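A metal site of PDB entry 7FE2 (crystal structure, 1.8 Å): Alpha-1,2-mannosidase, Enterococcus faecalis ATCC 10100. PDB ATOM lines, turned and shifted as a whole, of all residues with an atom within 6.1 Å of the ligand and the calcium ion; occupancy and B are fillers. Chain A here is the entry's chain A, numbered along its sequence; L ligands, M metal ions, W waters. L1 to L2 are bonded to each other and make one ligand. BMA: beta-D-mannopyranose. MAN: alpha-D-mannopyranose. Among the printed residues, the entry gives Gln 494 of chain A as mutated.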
ATOM      1  N   ASN A  22      25.063 -11.614  -7.253  1.00  0.00           N
ATOM      2  CA  ASN A  22      24.383 -10.301  -7.254  1.00  0.00           C
ATOM      3  C   ASN A  22      22.964 -10.499  -7.774  1.00  0.00           C
ATOM      4  O   ASN A  22      22.452  -9.613  -8.485  1.00  0.00           O
ATOM      5  CB  ASN A  22      25.225  -9.258  -8.030  1.00  0.00           C
ATOM      6  CG  ASN A  22      26.045  -8.393  -7.087  1.00  0.00           C
ATOM      7  OD1 ASN A  22      25.585  -8.077  -5.988  1.00  0.00           O
ATOM      8  ND2 ASN A  22      27.212  -7.987  -7.510  1.00  0.00           N
ATOM      9  N   PRO A  65      17.626  -4.925 -12.434  1.00  0.00           N
ATOM     10  CA  PRO A  65      18.267  -6.072 -13.067  1.00  0.00           C
ATOM     11  C   PRO A  65      19.589  -6.476 -12.401  1.00  0.00           C
ATOM     12  O   PRO A  65      20.063  -7.519 -12.724  1.00  0.00           O
ATOM     13  CB  PRO A  65      18.563  -5.584 -14.490  1.00  0.00           C
ATOM     14  CG  PRO A  65      18.831  -4.089 -14.311  1.00  0.00           C
ATOM     15  CD  PRO A  65      17.957  -3.674 -13.141  1.00  0.00           C
ATOM     16  N   SER A  66      20.207  -5.550 -11.651  1.00  0.00           N
ATOM     17  CA  SER A  66      21.573  -5.670 -11.078  1.00  0.00           C
ATOM     18  C   SER A  66      21.771  -4.457 -10.180  1.00  0.00           C
ATOM     19  O   SER A  66      21.097  -3.426 -10.323  1.00  0.00           O
ATOM     20  CB  SER A  66      22.645  -5.761 -12.139  1.00  0.00           C
ATOM     21  OG  SER A  66      23.102  -4.491 -12.536  1.00  0.00           O
ATOM     22  N   PRO A  67      22.694  -4.522  -9.220  1.00  0.00           N
ATOM     23  CA  PRO A  67      22.887  -3.417  -8.283  1.00  0.00           C
ATOM     24  C   PRO A  67      23.636  -2.266  -8.957  1.00  0.00           C
ATOM     25  O   PRO A  67      23.608  -1.141  -8.452  1.00  0.00           O
ATOM     26  CB  PRO A  67      23.714  -4.061  -7.146  1.00  0.00           C
ATOM     27  CG  PRO A  67      24.449  -5.186  -7.788  1.00  0.00           C
ATOM     28  CD  PRO A  67      23.595  -5.657  -8.937  1.00  0.00           C
ATOM     29  N   TRP A  68      24.277  -2.550 -10.083  1.00  0.00           N
ATOM     30  CA  TRP A  68      25.045  -1.581 -10.883  1.00  0.00           C
ATOM     31  C   TRP A  68      24.102  -0.680 -11.687  1.00  0.00           C
ATOM     32  O   TRP A  68      24.420   0.492 -11.894  1.00  0.00           O
ATOM     33  CB  TRP A  68      26.031  -2.333 -11.790  1.00  0.00           C
ATOM     34  CG  TRP A  68      26.828  -3.338 -11.005  1.00  0.00           C
ATOM     35  CD1 TRP A  68      26.699  -4.693 -11.107  1.00  0.00           C
ATOM     36  CD2 TRP A  68      27.686  -3.099  -9.878  1.00  0.00           C
ATOM     37  NE1 TRP A  68      27.482  -5.324 -10.159  1.00  0.00           N
ATOM     38  CE2 TRP A  68      28.093  -4.375  -9.381  1.00  0.00           C
ATOM     39  CE3 TRP A  68      28.235  -1.966  -9.286  1.00  0.00           C
ATOM     40  CZ2 TRP A  68      28.961  -4.532  -8.314  1.00  0.00           C
ATOM     41  CZ3 TRP A  68      29.132  -2.126  -8.253  1.00  0.00           C
ATOM     42  CH2 TRP A  68      29.463  -3.383  -7.746  1.00  0.00           C
ATOM     43  N   MET A  69      23.024  -1.242 -12.192  1.00  0.00           N
ATOM     44  CA  MET A  69      22.012  -0.473 -12.993  1.00  0.00           C
ATOM     45  C   MET A  69      21.073   0.225 -12.018  1.00  0.00           C
ATOM     46  O   MET A  69      20.517   1.259 -12.379  1.00  0.00           O
ATOM     47  CB  MET A  69      21.215  -1.388 -13.936  1.00  0.00           C
ATOM     48  CG  MET A  69      22.070  -2.134 -14.981  1.00  0.00           C
ATOM     49  SD  MET A  69      23.315  -1.097 -15.796  1.00  0.00           S
ATOM     50  CE  MET A  69      22.137  -0.007 -16.562  1.00  0.00           C
ATOM     51  N   GLY A 310      21.677  -6.392 -20.694  1.00  0.00           N
ATOM     52  CA  GLY A 310      22.942  -5.937 -21.261  1.00  0.00           C
ATOM     53  C   GLY A 310      23.472  -7.000 -22.200  1.00  0.00           C
ATOM     54  O   GLY A 310      23.984  -8.054 -21.703  1.00  0.00           O
ATOM     55  N   TRP A 312      26.144  -7.335 -23.862  1.00  0.00           N
ATOM     56  CA  TRP A 312      27.545  -7.704 -23.509  1.00  0.00           C
ATOM     57  C   TRP A 312      27.546  -9.000 -22.681  1.00  0.00           C
ATOM     58  O   TRP A 312      28.435  -9.825 -22.881  1.00  0.00           O
ATOM     59  CB  TRP A 312      28.218  -6.546 -22.763  1.00  0.00           C
ATOM     60  CG  TRP A 312      29.697  -6.642 -22.515  1.00  0.00           C
ATOM     61  CD1 TRP A 312      30.681  -6.183 -23.353  1.00  0.00           C
ATOM     62  CD2 TRP A 312      30.364  -7.134 -21.339  1.00  0.00           C
ATOM     63  NE1 TRP A 312      31.917  -6.386 -22.787  1.00  0.00           N
ATOM     64  CE2 TRP A 312      31.752  -6.947 -21.542  1.00  0.00           C
ATOM     65  CE3 TRP A 312      29.943  -7.713 -20.138  1.00  0.00           C
ATOM     66  CZ2 TRP A 312      32.713  -7.334 -20.598  1.00  0.00           C
ATOM     67  CZ3 TRP A 312      30.884  -8.101 -19.199  1.00  0.00           C
ATOM     68  CH2 TRP A 312      32.248  -7.907 -19.430  1.00  0.00           C
ATOM     69  N   ASP A 313      26.589  -9.162 -21.787  1.00  0.00           N
ATOM     70  CA  ASP A 313      26.390 -10.370 -20.955  1.00  0.00           C
ATOM     71  C   ASP A 313      25.554 -11.458 -21.678  1.00  0.00           C
ATOM     72  O   ASP A 313      25.998 -12.601 -21.751  1.00  0.00           O
ATOM     73  CB  ASP A 313      25.633 -10.024 -19.667  1.00  0.00           C
ATOM     74  CG  ASP A 313      26.250  -8.939 -18.815  1.00  0.00           C
ATOM     75  OD1 ASP A 313      27.477  -8.984 -18.637  1.00  0.00           O
ATOM     76  OD2 ASP A 313      25.450  -8.065 -18.284  1.00  0.00           O
ATOM     77  N   TRP A 350      22.277  -1.595 -23.458  1.00  0.00           N
ATOM     78  CA  TRP A 350      21.937  -1.934 -22.047  1.00  0.00           C
ATOM     79  C   TRP A 350      20.592  -1.278 -21.735  1.00  0.00           C
ATOM     80  O   TRP A 350      20.564  -0.064 -21.486  1.00  0.00           O
ATOM     81  CB  TRP A 350      23.026  -1.521 -21.040  1.00  0.00           C
ATOM     82  CG  TRP A 350      23.372  -2.564 -20.018  1.00  0.00           C
ATOM     83  CD1 TRP A 350      24.582  -3.182 -19.851  1.00  0.00           C
ATOM     84  CD2 TRP A 350      22.488  -3.214 -19.098  1.00  0.00           C
ATOM     85  NE1 TRP A 350      24.518  -4.124 -18.860  1.00  0.00           N
ATOM     86  CE2 TRP A 350      23.244  -4.187 -18.399  1.00  0.00           C
ATOM     87  CE3 TRP A 350      21.124  -3.114 -18.829  1.00  0.00           C
ATOM     88  CZ2 TRP A 350      22.679  -5.029 -17.443  1.00  0.00           C
ATOM     89  CZ3 TRP A 350      20.570  -3.937 -17.881  1.00  0.00           C
ATOM     90  CH2 TRP A 350      21.332  -4.901 -17.203  1.00  0.00           C
ATOM     91  N   LEU A 358      25.878   1.213 -21.085  1.00  0.00           N
ATOM     92  CA  LEU A 358      26.994   0.709 -20.247  1.00  0.00           C
ATOM     93  C   LEU A 358      27.591  -0.543 -20.935  1.00  0.00           C
ATOM     94  O   LEU A 358      26.864  -1.268 -21.658  1.00  0.00           O
ATOM     95  CB  LEU A 358      26.494   0.429 -18.821  1.00  0.00           C
ATOM     96  CG  LEU A 358      27.565   0.051 -17.787  1.00  0.00           C
ATOM     97  CD1 LEU A 358      28.186   1.291 -17.133  1.00  0.00           C
ATOM     98  CD2 LEU A 358      26.971  -0.862 -16.709  1.00  0.00           C
ATOM     99  N   MET A 359      28.905  -0.707 -20.757  1.00  0.00           N
ATOM    100  CA  MET A 359      29.762  -1.836 -21.232  1.00  0.00           C
ATOM    101  C   MET A 359      30.183  -1.568 -22.667  1.00  0.00           C
ATOM    102  O   MET A 359      29.493  -0.859 -23.421  1.00  0.00           O
ATOM    103  CB  MET A 359      29.082  -3.212 -21.113  1.00  0.00           C
ATOM    104  CG  MET A 359      28.636  -3.562 -19.688  1.00  0.00           C
ATOM    105  SD  MET A 359      29.944  -3.176 -18.446  1.00  0.00           S
ATOM    106  CE  MET A 359      31.189  -4.429 -18.800  1.00  0.00           C
ATOM    107  N   GLN A 494      37.301  -4.544 -17.076  1.00  0.00           N
ATOM    108  CA  GLN A 494      37.028  -5.522 -15.992  1.00  0.00           C
ATOM    109  C   GLN A 494      37.941  -6.737 -16.186  1.00  0.00           C
ATOM    110  O   GLN A 494      37.447  -7.867 -16.028  1.00  0.00           O
ATOM    111  CB  GLN A 494      35.550  -5.926 -15.971  1.00  0.00           C
ATOM    112  CG  GLN A 494      34.629  -4.708 -15.986  1.00  0.00           C
ATOM    113  CD  GLN A 494      33.173  -5.037 -15.779  1.00  0.00           C
ATOM    114  OE1 GLN A 494      32.745  -6.202 -15.829  1.00  0.00           O
ATOM    115  NE2 GLN A 494      32.401  -3.986 -15.545  1.00  0.00           N
ATOM    116  N   TYR A 540      42.461   0.964 -12.367  1.00  0.00           N
ATOM    117  CA  TYR A 540      41.286   1.364 -11.554  1.00  0.00           C
ATOM    118  C   TYR A 540      41.708   2.290 -10.398  1.00  0.00           C
ATOM    119  O   TYR A 540      40.942   3.256 -10.094  1.00  0.00           O
ATOM    120  CB  TYR A 540      40.528   0.117 -11.072  1.00  0.00           C
ATOM    121  CG  TYR A 540      39.681  -0.539 -12.142  1.00  0.00           C
ATOM    122  CD1 TYR A 540      38.354  -0.166 -12.341  1.00  0.00           C
ATOM    123  CD2 TYR A 540      40.185  -1.561 -12.945  1.00  0.00           C
ATOM    124  CE1 TYR A 540      37.564  -0.783 -13.316  1.00  0.00           C
ATOM    125  CE2 TYR A 540      39.403  -2.197 -13.907  1.00  0.00           C
ATOM    126  CZ  TYR A 540      38.097  -1.784 -14.113  1.00  0.00           C
ATOM    127  OH  TYR A 540      37.321  -2.399 -15.064  1.00  0.00           O
ATOM    128  N   ILE A 544      38.524  -4.039  -7.325  1.00  0.00           N
ATOM    129  CA  ILE A 544      37.081  -4.170  -7.639  1.00  0.00           C
ATOM    130  C   ILE A 544      36.680  -5.638  -7.471  1.00  0.00           C
ATOM    131  O   ILE A 544      37.572  -6.530  -7.511  1.00  0.00           O
ATOM    132  CB  ILE A 544      36.777  -3.672  -9.063  1.00  0.00           C
ATOM    133  CG1 ILE A 544      37.455  -4.532 -10.124  1.00  0.00           C
ATOM    134  CG2 ILE A 544      37.104  -2.202  -9.188  1.00  0.00           C
ATOM    135  CD1 ILE A 544      37.095  -4.126 -11.556  1.00  0.00           C
ATOM    136  N   HIS A 545      35.414  -5.862  -7.254  1.00  0.00           N
ATOM    137  CA  HIS A 545      34.889  -7.206  -6.901  1.00  0.00           C
ATOM    138  C   HIS A 545      35.322  -8.250  -7.949  1.00  0.00           C
ATOM    139  O   HIS A 545      35.589  -9.385  -7.531  1.00  0.00           O
ATOM    140  CB  HIS A 545      33.384  -7.136  -6.604  1.00  0.00           C
ATOM    141  CG  HIS A 545      32.508  -7.009  -7.795  1.00  0.00           C
ATOM    142  ND1 HIS A 545      31.922  -8.114  -8.409  1.00  0.00           N
ATOM    143  CD2 HIS A 545      32.096  -5.920  -8.486  1.00  0.00           C
ATOM    144  CE1 HIS A 545      31.112  -7.687  -9.379  1.00  0.00           C
ATOM    145  NE2 HIS A 545      31.243  -6.368  -9.481  1.00  0.00           N
ATOM    146  N   GLU A 546      35.377  -7.927  -9.256  1.00  0.00           N
ATOM    147  CA  GLU A 546      35.786  -8.940 -10.292  1.00  0.00           C
ATOM    148  C   GLU A 546      37.207  -9.447 -10.037  1.00  0.00           C
ATOM    149  O   GLU A 546      37.493 -10.591 -10.339  1.00  0.00           O
ATOM    150  CB  GLU A 546      35.692  -8.387 -11.697  1.00  0.00           C
ATOM    151  CG  GLU A 546      34.245  -8.242 -12.199  1.00  0.00           C
ATOM    152  CD  GLU A 546      33.565  -6.915 -11.922  1.00  0.00           C
ATOM    153  OE1 GLU A 546      32.464  -6.684 -12.537  1.00  0.00           O
ATOM    154  OE2 GLU A 546      34.142  -6.089 -11.153  1.00  0.00           O
ATOM    155  N   SER A 561      34.300 -15.843 -12.971  1.00  0.00           N
ATOM    156  CA  SER A 561      33.426 -14.857 -12.292  1.00  0.00           C
ATOM    157  C   SER A 561      32.907 -13.762 -13.249  1.00  0.00           C
ATOM    158  O   SER A 561      31.979 -13.011 -12.846  1.00  0.00           O
ATOM    159  CB  SER A 561      34.200 -14.216 -11.136  1.00  0.00           C
ATOM    160  OG  SER A 561      35.462 -13.763 -11.611  1.00  0.00           O
ATOM    161  N   ASN A 562      33.460 -13.632 -14.453  1.00  0.00           N
ATOM    162  CA  ASN A 562      33.058 -12.562 -15.378  1.00  0.00           C
ATOM    163  C   ASN A 562      33.024 -13.095 -16.816  1.00  0.00           C
ATOM    164  O   ASN A 562      33.793 -14.025 -17.175  1.00  0.00           O
ATOM    165  CB  ASN A 562      33.984 -11.340 -15.224  1.00  0.00           C
ATOM    166  CG  ASN A 562      33.381 -10.046 -15.722  1.00  0.00           C
ATOM    167  OD1 ASN A 562      32.164  -9.912 -15.790  1.00  0.00           O
ATOM    168  ND2 ASN A 562      34.234  -9.073 -16.012  1.00  0.00           N
ATOM    169  N   GLN A 563      32.199 -12.455 -17.641  1.00  0.00           N
ATOM    170  CA  GLN A 563      31.882 -12.878 -19.037  1.00  0.00           C
ATOM    171  C   GLN A 563      33.107 -13.042 -19.918  1.00  0.00           C
ATOM    172  O   GLN A 563      33.098 -13.954 -20.750  1.00  0.00           O
ATOM    173  CB  GLN A 563      30.898 -11.905 -19.692  1.00  0.00           C
ATOM    174  CG  GLN A 563      29.466 -12.198 -19.305  1.00  0.00           C
ATOM    175  CD  GLN A 563      29.173 -11.705 -17.918  1.00  0.00           C
ATOM    176  OE1 GLN A 563      29.880 -10.865 -17.376  1.00  0.00           O
ATOM    177  NE2 GLN A 563      28.113 -12.236 -17.333  1.00  0.00           N
ATOM    178  N   PRO A 564      34.150 -12.195 -19.839  1.00  0.00           N
ATOM    179  CA  PRO A 564      35.305 -12.291 -20.743  1.00  0.00           C
ATOM    180  C   PRO A 564      35.996 -13.657 -20.776  1.00  0.00           C
ATOM    181  O   PRO A 564      36.425 -14.013 -21.869  1.00  0.00           O
ATOM    182  CB  PRO A 564      36.265 -11.191 -20.259  1.00  0.00           C
ATOM    183  CG  PRO A 564      35.343 -10.207 -19.592  1.00  0.00           C
ATOM    184  CD  PRO A 564      34.300 -11.060 -18.905  1.00  0.00           C
ATOM    185  N   ASP A 602      28.973 -12.280 -10.826  1.00  0.00           N
ATOM    186  CA  ASP A 602      27.658 -11.689 -11.184  1.00  0.00           C
ATOM    187  C   ASP A 602      26.931 -12.589 -12.203  1.00  0.00           C
ATOM    188  O   ASP A 602      27.538 -13.005 -13.214  1.00  0.00           O
ATOM    189  CB  ASP A 602      27.786 -10.301 -11.768  1.00  0.00           C
ATOM    190  CG  ASP A 602      28.080  -9.226 -10.741  1.00  0.00           C
ATOM    191  OD1 ASP A 602      28.409  -9.534  -9.563  1.00  0.00           O
ATOM    192  OD2 ASP A 602      27.950  -8.106 -11.122  1.00  0.00           O
ATOM    193  N   ASP A 604      24.291 -11.792 -13.907  1.00  0.00           N
ATOM    194  CA  ASP A 604      23.962 -10.913 -15.088  1.00  0.00           C
ATOM    195  C   ASP A 604      22.802 -11.467 -15.957  1.00  0.00           C
ATOM    196  O   ASP A 604      23.012 -11.756 -17.175  1.00  0.00           O
ATOM    197  CB  ASP A 604      25.219 -10.710 -15.907  1.00  0.00           C
ATOM    198  CG  ASP A 604      26.296  -9.899 -15.193  1.00  0.00           C
ATOM    199  OD1 ASP A 604      25.948  -8.852 -14.600  1.00  0.00           O
ATOM    200  OD2 ASP A 604      27.463 -10.353 -15.206  1.00  0.00           O
ATOM    201  N   ASN A 605      21.577 -11.462 -15.416  1.00  0.00           N
ATOM    202  CA  ASN A 605      20.297 -11.566 -16.166  1.00  0.00           C
ATOM    203  C   ASN A 605      20.291 -12.807 -17.085  1.00  0.00           C
ATOM    204  O   ASN A 605      19.907 -12.681 -18.262  1.00  0.00           O
ATOM    205  CB  ASN A 605      20.115 -10.259 -16.939  1.00  0.00           C
ATOM    206  CG  ASN A 605      20.299  -9.085 -16.020  1.00  0.00           C
ATOM    207  OD1 ASN A 605      21.262  -8.336 -16.140  1.00  0.00           O
ATOM    208  ND2 ASN A 605      19.406  -8.939 -15.062  1.00  0.00           N
HETATM  209  C1  BMA L   1      29.943  -1.924 -13.084  1.00  0.00           C
HETATM  210  C2  BMA L   1      29.727  -3.405 -12.867  1.00  0.00           C
HETATM  211  C3  BMA L   1      30.680  -3.859 -11.764  1.00  0.00           C
HETATM  212  C4  BMA L   1      32.123  -3.444 -12.013  1.00  0.00           C
HETATM  213  C5  BMA L   1      32.228  -2.006 -12.473  1.00  0.00           C
HETATM  214  C6  BMA L   1      33.595  -1.690 -13.054  1.00  0.00           C
HETATM  215  O1  BMA L   1      29.050  -1.452 -14.100  1.00  0.00           O
HETATM  216  O2  BMA L   1      30.071  -4.141 -14.056  1.00  0.00           O
HETATM  217  O3  BMA L   1      30.590  -5.276 -11.644  1.00  0.00           O
HETATM  218  O4  BMA L   1      32.932  -3.696 -10.860  1.00  0.00           O
HETATM  219  O5  BMA L   1      31.295  -1.776 -13.500  1.00  0.00           O
HETATM  220  O6  BMA L   1      33.928  -0.344 -12.742  1.00  0.00           O
HETATM  221  C1  MAN L   2      29.089  -4.990 -14.649  1.00  0.00           C
HETATM  222  C2  MAN L   2      29.582  -5.986 -15.737  1.00  0.00           C
HETATM  223  C3  MAN L   2      28.455  -6.454 -16.667  1.00  0.00           C
HETATM  224  C4  MAN L   2      27.031  -5.863 -16.400  1.00  0.00           C
HETATM  225  C5  MAN L   2      27.004  -4.474 -15.740  1.00  0.00           C
HETATM  226  C6  MAN L   2      25.643  -3.938 -15.307  1.00  0.00           C
HETATM  227  O2  MAN L   2      30.277  -7.201 -15.283  1.00  0.00           O
HETATM  228  O3  MAN L   2      28.653  -7.886 -16.543  1.00  0.00           O
HETATM  229  O4  MAN L   2      26.304  -5.799 -17.641  1.00  0.00           O
HETATM  230  O5  MAN L   2      27.711  -4.641 -14.527  1.00  0.00           O
HETATM  231  O6  MAN L   2      24.922  -4.863 -14.458  1.00  0.00           O
HETATM  232 CA    CA M   1      29.749  -9.523 -15.216  1.00  0.00          CA
HETATM  233  O   HOH W   1      33.153  -2.344  -8.547  1.00  0.00           O
HETATM  234  O   HOH W   2      23.870  -7.250 -15.195  1.00  0.00           O
HETATM  235  O   HOH W   3      29.822 -11.838 -14.112  1.00  0.00           O
HETATM  236  O   HOH W   4      28.044  -7.640 -13.850  1.00  0.00           O
HETATM  237  O   HOH W   5      30.865  -8.879 -13.142  1.00  0.00           O
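Three residues have an atom within 4 Å of the calcium ion: Asn 562, Gln 563 and Asp 604.
The calcium ion is bound by O3 of MAN L2, 2.4 Å away. O2 of MAN L2 is bound to the calcium ion (2.4 Å). The calcium ion is bound by the side-chain carboxylate (OD2) of Asp 604. Water W5 binds the calcium ion. The calcium ion is bound by the side-chain amide oxygen (OD1) of Asn 562 (2.5 Å). The calcium ion is bound by the side-chain amide oxygen (OE1) of Gln 563, at 2.5 Å. Water W3 is bound to the calcium ion, 2.6 Å away. Water W4 is bound to the calcium ion (2.9 Å).
Water W3 lies within hydrogen-bond range of the backbone carbonyl oxygen of Asp 602 (2.7 Å) and the backbone carbonyl oxygen of Ser 561 (2.8 Å). Water W2 lies within hydrogen-bond range of OD1 of Asp 604, O6 of MAN L2 and OD1 of Asn 605.
OD1 of Asp 313 lies close to OE1 of Gln 563 (3.3 Å). The side-chain amide oxygen of Gln 494 lies close to the side-chain carboxylate of Glu 546, at 3.3 Å. ND2 of Asn 562 is in hydrogen-bond range of OE1 of Gln 494, 3.2 Å away. The side-chain hydroxyl of Ser 66 sits close to the backbone NH of Trp 68. The side-chain hydroxyl of Ser 66 sits at hydrogen-bond distance from the backbone NH of Met 69 (3.3 Å). The backbone NH of Gln 494 lies within hydrogen-bond range of the side-chain hydroxyl of Tyr 540 (2.9 Å). NE1 of Trp 68 is in hydrogen-bond range of OD2 of Asp 602 (3.0 Å). The side-chain carboxylate (OD1) of Asp 602 lies within hydrogen-bond range of the side-chain amide nitrogen (ND2) of Asn 22.
An oxygen (O4) of MAN L2 is in hydrogen-bond range of the side-chain carboxylate (OD2) of Asp 313. The side-chain carboxylate (OE1) of Glu 546 lies within hydrogen-bond range of an oxygen (O3) of BMA L1. A ring nitrogen (NE2) of His 545 sits at hydrogen-bond distance from an oxygen (O3) of BMA L1, 2.5 Å away. OG of Ser 66 lies within hydrogen-bond range of O6 of MAN L2, at 2.7 Å. The side-chain amide nitrogen (NE2) of Gln 494 lies within hydrogen-bond range of an oxygen (O2) of BMA L1 (2.8 Å). The indole nitrogen of Trp 350 sits at hydrogen-bond distance from an oxygen (O4) of MAN L2, at 2.7 Å. NE1 of Trp 68 sits at hydrogen-bond distance from O3 of BMA L1.
Merely in contact with the ligand: Met 69 (3.7 Å), Trp 312 (3.5 Å), Leu 358 (3.4 Å), Met 359 (3.8 Å), Tyr 540 (3.7 Å) and Asp 602 (3.9 Å). 16 residues have an atom within 4 Å of the ligand: Ser 66, Trp 68, Met 69, Trp 312, Asp 313, Trp 350, Leu 358, Met 359, Gln 494, Tyr 540, His 545, Glu 546, Asn 562, Gln 563, Asp 602 and Asp 604. The nearest printed residue that does not touch the ligand is Ile 544 (4.2 Å).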
